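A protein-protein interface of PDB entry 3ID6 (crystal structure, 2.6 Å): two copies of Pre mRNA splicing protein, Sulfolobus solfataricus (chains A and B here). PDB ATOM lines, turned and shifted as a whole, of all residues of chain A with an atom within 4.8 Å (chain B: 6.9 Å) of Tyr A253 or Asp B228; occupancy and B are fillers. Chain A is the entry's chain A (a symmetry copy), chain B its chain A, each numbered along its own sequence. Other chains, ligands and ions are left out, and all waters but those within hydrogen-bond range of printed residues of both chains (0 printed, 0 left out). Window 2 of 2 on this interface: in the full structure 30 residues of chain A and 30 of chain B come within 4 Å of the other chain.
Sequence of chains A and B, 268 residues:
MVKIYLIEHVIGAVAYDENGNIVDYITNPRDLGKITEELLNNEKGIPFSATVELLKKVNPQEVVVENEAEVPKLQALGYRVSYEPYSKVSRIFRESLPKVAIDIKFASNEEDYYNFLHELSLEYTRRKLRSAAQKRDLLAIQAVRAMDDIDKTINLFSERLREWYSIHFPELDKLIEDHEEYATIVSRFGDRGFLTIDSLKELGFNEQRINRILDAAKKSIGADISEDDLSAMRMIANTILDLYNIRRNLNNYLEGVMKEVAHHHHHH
OD2 of Asp B229 sits at hydrogen-bond distance from OH of Tyr A253.
OG of Ser B226 is in hydrogen-bond range of OD1 of Asp B229.
Among the printed residues, merely in contact across the chains: Leu A139 with Trp B164 (3.9 Å), Leu A139 with Asp B229 (3.6 Å), Leu A139 with Met B233 (3.8 Å), Asn A249 with Met B235 (3.6 Å), Leu A250 with Trp B164 (3.9 Å), Leu A250 with Ala B232 (3.8 Å), Tyr A253 with Asp B228 (3.6 Å) and Tyr A253 with Ala B232 (3.96 Å).
Asp B228 touches one residue of chain A. Of the printed residues of chain A, Met B235 touches Asn A249. Of the printed residues of chain A, Met B233 touches Leu A139 (3.8 Å). Of the printed residues of chain B, Leu A250 touches Trp B164 (3.9 Å) and Ala B232 (3.8 Å). The nearest residue of chain B that does not touch Tyr A253 is Trp B164 (4.5 Å). The nearest printed residue of chain A that does not touch Asp B228 is Val A257 (5.9 Å). The nearest printed residue of chain A that does not touch Asp B229 is Val A257 (4.7 Å).
Of the 11 printed residues of chain A, 4 touch a printed residue of chain B. Of the 11 printed residues of chain B, 6 touch a printed residue of chain A. Printed residues of chain B that touch a printed residue of chain A: Trp B164, Asp B228, Asp B229, Ala B232, Met B233 and Met B235.
No position is printed for both chains.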
ATOM      1  N   LEU A 139      12.996  -0.372  26.411  1.00  0.00           N
ATOM      2  CA  LEU A 139      12.979  -0.980  25.075  1.00  0.00           C
ATOM      3  C   LEU A 139      11.865  -0.399  24.220  1.00  0.00           C
ATOM      4  O   LEU A 139      11.997  -0.320  22.992  1.00  0.00           O
ATOM      5  CB  LEU A 139      12.850  -2.510  25.154  1.00  0.00           C
ATOM      6  CG  LEU A 139      14.016  -3.260  25.833  1.00  0.00           C
ATOM      7  CD1 LEU A 139      13.620  -4.686  26.254  1.00  0.00           C
ATOM      8  CD2 LEU A 139      15.272  -3.279  24.959  1.00  0.00           C
ATOM      9  N   ALA A 143      11.845   1.691  20.473  1.00  0.00           N
ATOM     10  CA  ALA A 143      10.941   1.361  19.389  1.00  0.00           C
ATOM     11  C   ALA A 143      10.154   2.578  18.927  1.00  0.00           C
ATOM     12  O   ALA A 143       9.928   2.744  17.734  1.00  0.00           O
ATOM     13  CB  ALA A 143       9.987   0.257  19.809  1.00  0.00           C
ATOM     14  N   ASN A 249       5.788  -3.393  11.438  1.00  0.00           N
ATOM     15  CA  ASN A 249       6.301  -4.444  12.342  1.00  0.00           C
ATOM     16  C   ASN A 249       6.744  -3.940  13.708  1.00  0.00           C
ATOM     17  O   ASN A 249       6.670  -4.662  14.701  1.00  0.00           O
ATOM     18  CB  ASN A 249       7.472  -5.197  11.702  1.00  0.00           C
ATOM     19  CG  ASN A 249       7.073  -5.968  10.448  1.00  0.00           C
ATOM     20  OD1 ASN A 249       5.925  -6.394  10.298  1.00  0.00           O
ATOM     21  ND2 ASN A 249       8.024  -6.152   9.545  1.00  0.00           N
ATOM     22  N   LEU A 250       7.222  -2.702  13.755  1.00  0.00           N
ATOM     23  CA  LEU A 250       7.619  -2.082  15.012  1.00  0.00           C
ATOM     24  C   LEU A 250       6.398  -1.695  15.816  1.00  0.00           C
ATOM     25  O   LEU A 250       6.406  -1.782  17.041  1.00  0.00           O
ATOM     26  CB  LEU A 250       8.533  -0.873  14.775  1.00  0.00           C
ATOM     27  CG  LEU A 250      10.023  -1.166  14.559  1.00  0.00           C
ATOM     28  CD1 LEU A 250      10.828   0.120  14.444  1.00  0.00           C
ATOM     29  CD2 LEU A 250      10.604  -2.051  15.657  1.00  0.00           C
ATOM     30  N   ASN A 251       5.337  -1.293  15.122  1.00  0.00           N
ATOM     31  CA  ASN A 251       4.080  -0.963  15.791  1.00  0.00           C
ATOM     32  C   ASN A 251       3.407  -2.186  16.402  1.00  0.00           C
ATOM     33  O   ASN A 251       2.770  -2.079  17.450  1.00  0.00           O
ATOM     34  CB  ASN A 251       3.117  -0.238  14.857  1.00  0.00           C
ATOM     35  CG  ASN A 251       2.054   0.525  15.615  1.00  0.00           C
ATOM     36  OD1 ASN A 251       0.900   0.108  15.676  1.00  0.00           O
ATOM     37  ND2 ASN A 251       2.442   1.635  16.228  1.00  0.00           N
ATOM     38  N   ASN A 252       3.536  -3.338  15.743  1.00  0.00           N
ATOM     39  CA  ASN A 252       3.080  -4.592  16.331  1.00  0.00           C
ATOM     40  C   ASN A 252       3.901  -4.915  17.574  1.00  0.00           C
ATOM     41  O   ASN A 252       3.332  -5.147  18.639  1.00  0.00           O
ATOM     42  CB  ASN A 252       3.106  -5.749  15.325  1.00  0.00           C
ATOM     43  CG  ASN A 252       2.047  -5.608  14.237  1.00  0.00           C
ATOM     44  OD1 ASN A 252       1.051  -4.894  14.404  1.00  0.00           O
ATOM     45  ND2 ASN A 252       2.259  -6.288  13.113  1.00  0.00           N
ATOM     46  N   TYR A 253       5.228  -4.886  17.451  1.00  0.00           N
ATOM     47  CA  TYR A 253       6.111  -5.070  18.606  1.00  0.00           C
ATOM     48  C   TYR A 253       5.753  -4.153  19.786  1.00  0.00           C
ATOM     49  O   TYR A 253       5.635  -4.614  20.922  1.00  0.00           O
ATOM     50  CB  TYR A 253       7.573  -4.875  18.206  1.00  0.00           C
ATOM     51  CG  TYR A 253       8.523  -4.882  19.371  1.00  0.00           C
ATOM     52  CD1 TYR A 253       9.056  -3.688  19.866  1.00  0.00           C
ATOM     53  CD2 TYR A 253       8.899  -6.079  19.985  1.00  0.00           C
ATOM     54  CE1 TYR A 253       9.931  -3.691  20.950  1.00  0.00           C
ATOM     55  CE2 TYR A 253       9.777  -6.088  21.059  1.00  0.00           C
ATOM     56  CZ  TYR A 253      10.286  -4.891  21.538  1.00  0.00           C
ATOM     57  OH  TYR A 253      11.151  -4.892  22.601  1.00  0.00           O
ATOM     58  N   LEU A 254       5.568  -2.866  19.488  1.00  0.00           N
ATOM     59  CA  LEU A 254       5.263  -1.835  20.481  1.00  0.00           C
ATOM     60  C   LEU A 254       3.965  -2.117  21.226  1.00  0.00           C
ATOM     61  O   LEU A 254       3.915  -1.984  22.447  1.00  0.00           O
ATOM     62  CB  LEU A 254       5.174  -0.465  19.812  1.00  0.00           C
ATOM     63  CG  LEU A 254       5.645   0.839  20.469  1.00  0.00           C
ATOM     64  CD1 LEU A 254       4.582   1.926  20.263  1.00  0.00           C
ATOM     65  CD2 LEU A 254       5.984   0.705  21.956  1.00  0.00           C
ATOM     66  N   GLU A 255       2.919  -2.511  20.505  1.00  0.00           N
ATOM     67  CA  GLU A 255       1.643  -2.844  21.148  1.00  0.00           C
ATOM     68  C   GLU A 255       1.767  -4.045  22.076  1.00  0.00           C
ATOM     69  O   GLU A 255       1.491  -3.933  23.274  1.00  0.00           O
ATOM     70  CB  GLU A 255       0.539  -3.087  20.121  1.00  0.00           C
ATOM     71  CG  GLU A 255       0.039  -1.817  19.464  1.00  0.00           C
ATOM     72  CD  GLU A 255      -0.893  -2.106  18.311  1.00  0.00           C
ATOM     73  OE1 GLU A 255      -2.005  -2.627  18.569  1.00  0.00           O
ATOM     74  OE2 GLU A 255      -0.512  -1.813  17.154  1.00  0.00           O
ATOM     75  N   GLY A 256       2.194  -5.180  21.522  1.00  0.00           N
ATOM     76  CA  GLY A 256       2.400  -6.403  22.299  1.00  0.00           C
ATOM     77  C   GLY A 256       3.201  -6.230  23.582  1.00  0.00           C
ATOM     78  O   GLY A 256       2.974  -6.945  24.551  1.00  0.00           O
ATOM     79  N   VAL A 257       4.124  -5.272  23.586  1.00  0.00           N
ATOM     80  CA  VAL A 257       5.035  -5.039  24.713  1.00  0.00           C
ATOM     81  C   VAL A 257       4.530  -3.967  25.689  1.00  0.00           C
ATOM     82  O   VAL A 257       4.656  -4.122  26.903  1.00  0.00           O
ATOM     83  CB  VAL A 257       6.469  -4.731  24.201  1.00  0.00           C
ATOM     84  CG1 VAL A 257       7.267  -3.868  25.180  1.00  0.00           C
ATOM     85  CG2 VAL A 257       7.201  -6.037  23.883  1.00  0.00           C
ATOM     86  N   TRP B 164      19.921   1.684  21.465  1.00  0.00           N
ATOM     87  CA  TRP B 164      18.910   0.663  21.690  1.00  0.00           C
ATOM     88  C   TRP B 164      19.603  -0.608  22.135  1.00  0.00           C
ATOM     89  O   TRP B 164      19.283  -1.159  23.185  1.00  0.00           O
ATOM     90  CB  TRP B 164      18.120   0.427  20.404  1.00  0.00           C
ATOM     91  CG  TRP B 164      16.880  -0.416  20.540  1.00  0.00           C
ATOM     92  CD1 TRP B 164      16.521  -1.184  21.617  1.00  0.00           C
ATOM     93  CD2 TRP B 164      15.863  -0.613  19.550  1.00  0.00           C
ATOM     94  NE1 TRP B 164      15.336  -1.820  21.360  1.00  0.00           N
ATOM     95  CE2 TRP B 164      14.904  -1.489  20.105  1.00  0.00           C
ATOM     96  CE3 TRP B 164      15.653  -0.120  18.255  1.00  0.00           C
ATOM     97  CZ2 TRP B 164      13.750  -1.898  19.405  1.00  0.00           C
ATOM     98  CZ3 TRP B 164      14.494  -0.527  17.552  1.00  0.00           C
ATOM     99  CH2 TRP B 164      13.570  -1.412  18.132  1.00  0.00           C
ATOM    100  N   ILE B 225      17.604 -10.022  27.413  1.00  0.00           N
ATOM    101  CA  ILE B 225      16.632  -9.588  26.431  1.00  0.00           C
ATOM    102  C   ILE B 225      15.980 -10.796  25.774  1.00  0.00           C
ATOM    103  O   ILE B 225      16.567 -11.865  25.742  1.00  0.00           O
ATOM    104  CB  ILE B 225      17.322  -8.617  25.448  1.00  0.00           C
ATOM    105  CG1 ILE B 225      17.097  -7.186  25.923  1.00  0.00           C
ATOM    106  CG2 ILE B 225      16.854  -8.793  24.029  1.00  0.00           C
ATOM    107  CD1 ILE B 225      18.039  -6.202  25.283  1.00  0.00           C
ATOM    108  N   SER B 226      14.753 -10.644  25.291  1.00  0.00           N
ATOM    109  CA  SER B 226      14.067 -11.760  24.650  1.00  0.00           C
ATOM    110  C   SER B 226      14.254 -11.743  23.141  1.00  0.00           C
ATOM    111  O   SER B 226      14.714 -10.758  22.580  1.00  0.00           O
ATOM    112  CB  SER B 226      12.586 -11.756  25.006  1.00  0.00           C
ATOM    113  OG  SER B 226      11.983 -10.529  24.650  1.00  0.00           O
ATOM    114  N   GLU B 227      13.888 -12.837  22.488  1.00  0.00           N
ATOM    115  CA  GLU B 227      14.043 -12.959  21.042  1.00  0.00           C
ATOM    116  C   GLU B 227      13.206 -11.957  20.243  1.00  0.00           C
ATOM    117  O   GLU B 227      13.616 -11.541  19.162  1.00  0.00           O
ATOM    118  CB  GLU B 227      13.803 -14.401  20.595  1.00  0.00           C
ATOM    119  CG  GLU B 227      15.065 -15.264  20.727  1.00  0.00           C
ATOM    120  CD  GLU B 227      14.771 -16.761  20.893  1.00  0.00           C
ATOM    121  OE1 GLU B 227      15.366 -17.570  20.135  1.00  0.00           O
ATOM    122  OE2 GLU B 227      13.956 -17.132  21.779  1.00  0.00           O
ATOM    123  N   ASP B 228      12.053 -11.565  20.781  1.00  0.00           N
ATOM    124  CA  ASP B 228      11.273 -10.463  20.221  1.00  0.00           C
ATOM    125  C   ASP B 228      11.982  -9.101  20.321  1.00  0.00           C
ATOM    126  O   ASP B 228      11.963  -8.325  19.373  1.00  0.00           O
ATOM    127  CB  ASP B 228       9.893 -10.389  20.880  1.00  0.00           C
ATOM    128  CG  ASP B 228       8.878 -11.311  20.224  1.00  0.00           C
ATOM    129  OD1 ASP B 228       9.175 -11.874  19.144  1.00  0.00           O
ATOM    130  OD2 ASP B 228       7.773 -11.475  20.791  1.00  0.00           O
ATOM    131  N   ASP B 229      12.590  -8.814  21.472  1.00  0.00           N
ATOM    132  CA  ASP B 229      13.397  -7.605  21.633  1.00  0.00           C
ATOM    133  C   ASP B 229      14.551  -7.500  20.599  1.00  0.00           C
ATOM    134  O   ASP B 229      14.652  -6.507  19.876  1.00  0.00           O
ATOM    135  CB  ASP B 229      13.946  -7.506  23.059  1.00  0.00           C
ATOM    136  CG  ASP B 229      12.854  -7.459  24.126  1.00  0.00           C
ATOM    137  OD1 ASP B 229      13.087  -8.043  25.218  1.00  0.00           O
ATOM    138  OD2 ASP B 229      11.784  -6.840  23.895  1.00  0.00           O
ATOM    139  N   LEU B 230      15.419  -8.515  20.539  1.00  0.00           N
ATOM    140  CA  LEU B 230      16.487  -8.579  19.524  1.00  0.00           C
ATOM    141  C   LEU B 230      15.927  -8.434  18.125  1.00  0.00           C
ATOM    142  O   LEU B 230      16.473  -7.715  17.300  1.00  0.00           O
ATOM    143  CB  LEU B 230      17.269  -9.901  19.593  1.00  0.00           C
ATOM    144  CG  LEU B 230      18.083 -10.197  20.857  1.00  0.00           C
ATOM    145  CD1 LEU B 230      18.769 -11.577  20.751  1.00  0.00           C
ATOM    146  CD2 LEU B 230      19.102  -9.084  21.202  1.00  0.00           C
ATOM    147  N   SER B 231      14.821  -9.123  17.875  1.00  0.00           N
ATOM    148  CA  SER B 231      14.205  -9.146  16.557  1.00  0.00           C
ATOM    149  C   SER B 231      13.896  -7.744  16.029  1.00  0.00           C
ATOM    150  O   SER B 231      14.249  -7.409  14.898  1.00  0.00           O
ATOM    151  CB  SER B 231      12.947  -9.987  16.596  1.00  0.00           C
ATOM    152  OG  SER B 231      12.519 -10.252  15.294  1.00  0.00           O
ATOM    153  N   ALA B 232      13.256  -6.935  16.872  1.00  0.00           N
ATOM    154  CA  ALA B 232      12.928  -5.556  16.558  1.00  0.00           C
ATOM    155  C   ALA B 232      14.185  -4.716  16.298  1.00  0.00           C
ATOM    156  O   ALA B 232      14.217  -3.939  15.327  1.00  0.00           O
ATOM    157  CB  ALA B 232      12.094  -4.956  17.672  1.00  0.00           C
ATOM    158  N   MET B 233      15.208  -4.876  17.145  1.00  0.00           N
ATOM    159  CA  MET B 233      16.497  -4.200  16.937  1.00  0.00           C
ATOM    160  C   MET B 233      17.100  -4.605  15.595  1.00  0.00           C
ATOM    161  O   MET B 233      17.695  -3.783  14.914  1.00  0.00           O
ATOM    162  CB  MET B 233      17.517  -4.531  18.042  1.00  0.00           C
ATOM    163  CG  MET B 233      17.163  -4.136  19.455  1.00  0.00           C
ATOM    164  SD  MET B 233      18.361  -4.891  20.599  1.00  0.00           S
ATOM    165  CE  MET B 233      17.537  -4.660  22.173  1.00  0.00           C
ATOM    166  N   MET B 235      15.595  -5.287  12.874  1.00  0.00           N
ATOM    167  CA  MET B 235      14.987  -4.588  11.760  1.00  0.00           C
ATOM    168  C   MET B 235      15.775  -3.325  11.418  1.00  0.00           C
ATOM    169  O   MET B 235      15.967  -3.025  10.233  1.00  0.00           O
ATOM    170  CB  MET B 235      13.514  -4.293  12.017  1.00  0.00           C
ATOM    171  CG  MET B 235      12.643  -5.550  12.061  1.00  0.00           C
ATOM    172  SD  MET B 235      10.958  -5.090  12.479  1.00  0.00           S
ATOM    173  CE  MET B 235      10.488  -6.468  13.547  1.00  0.00           C
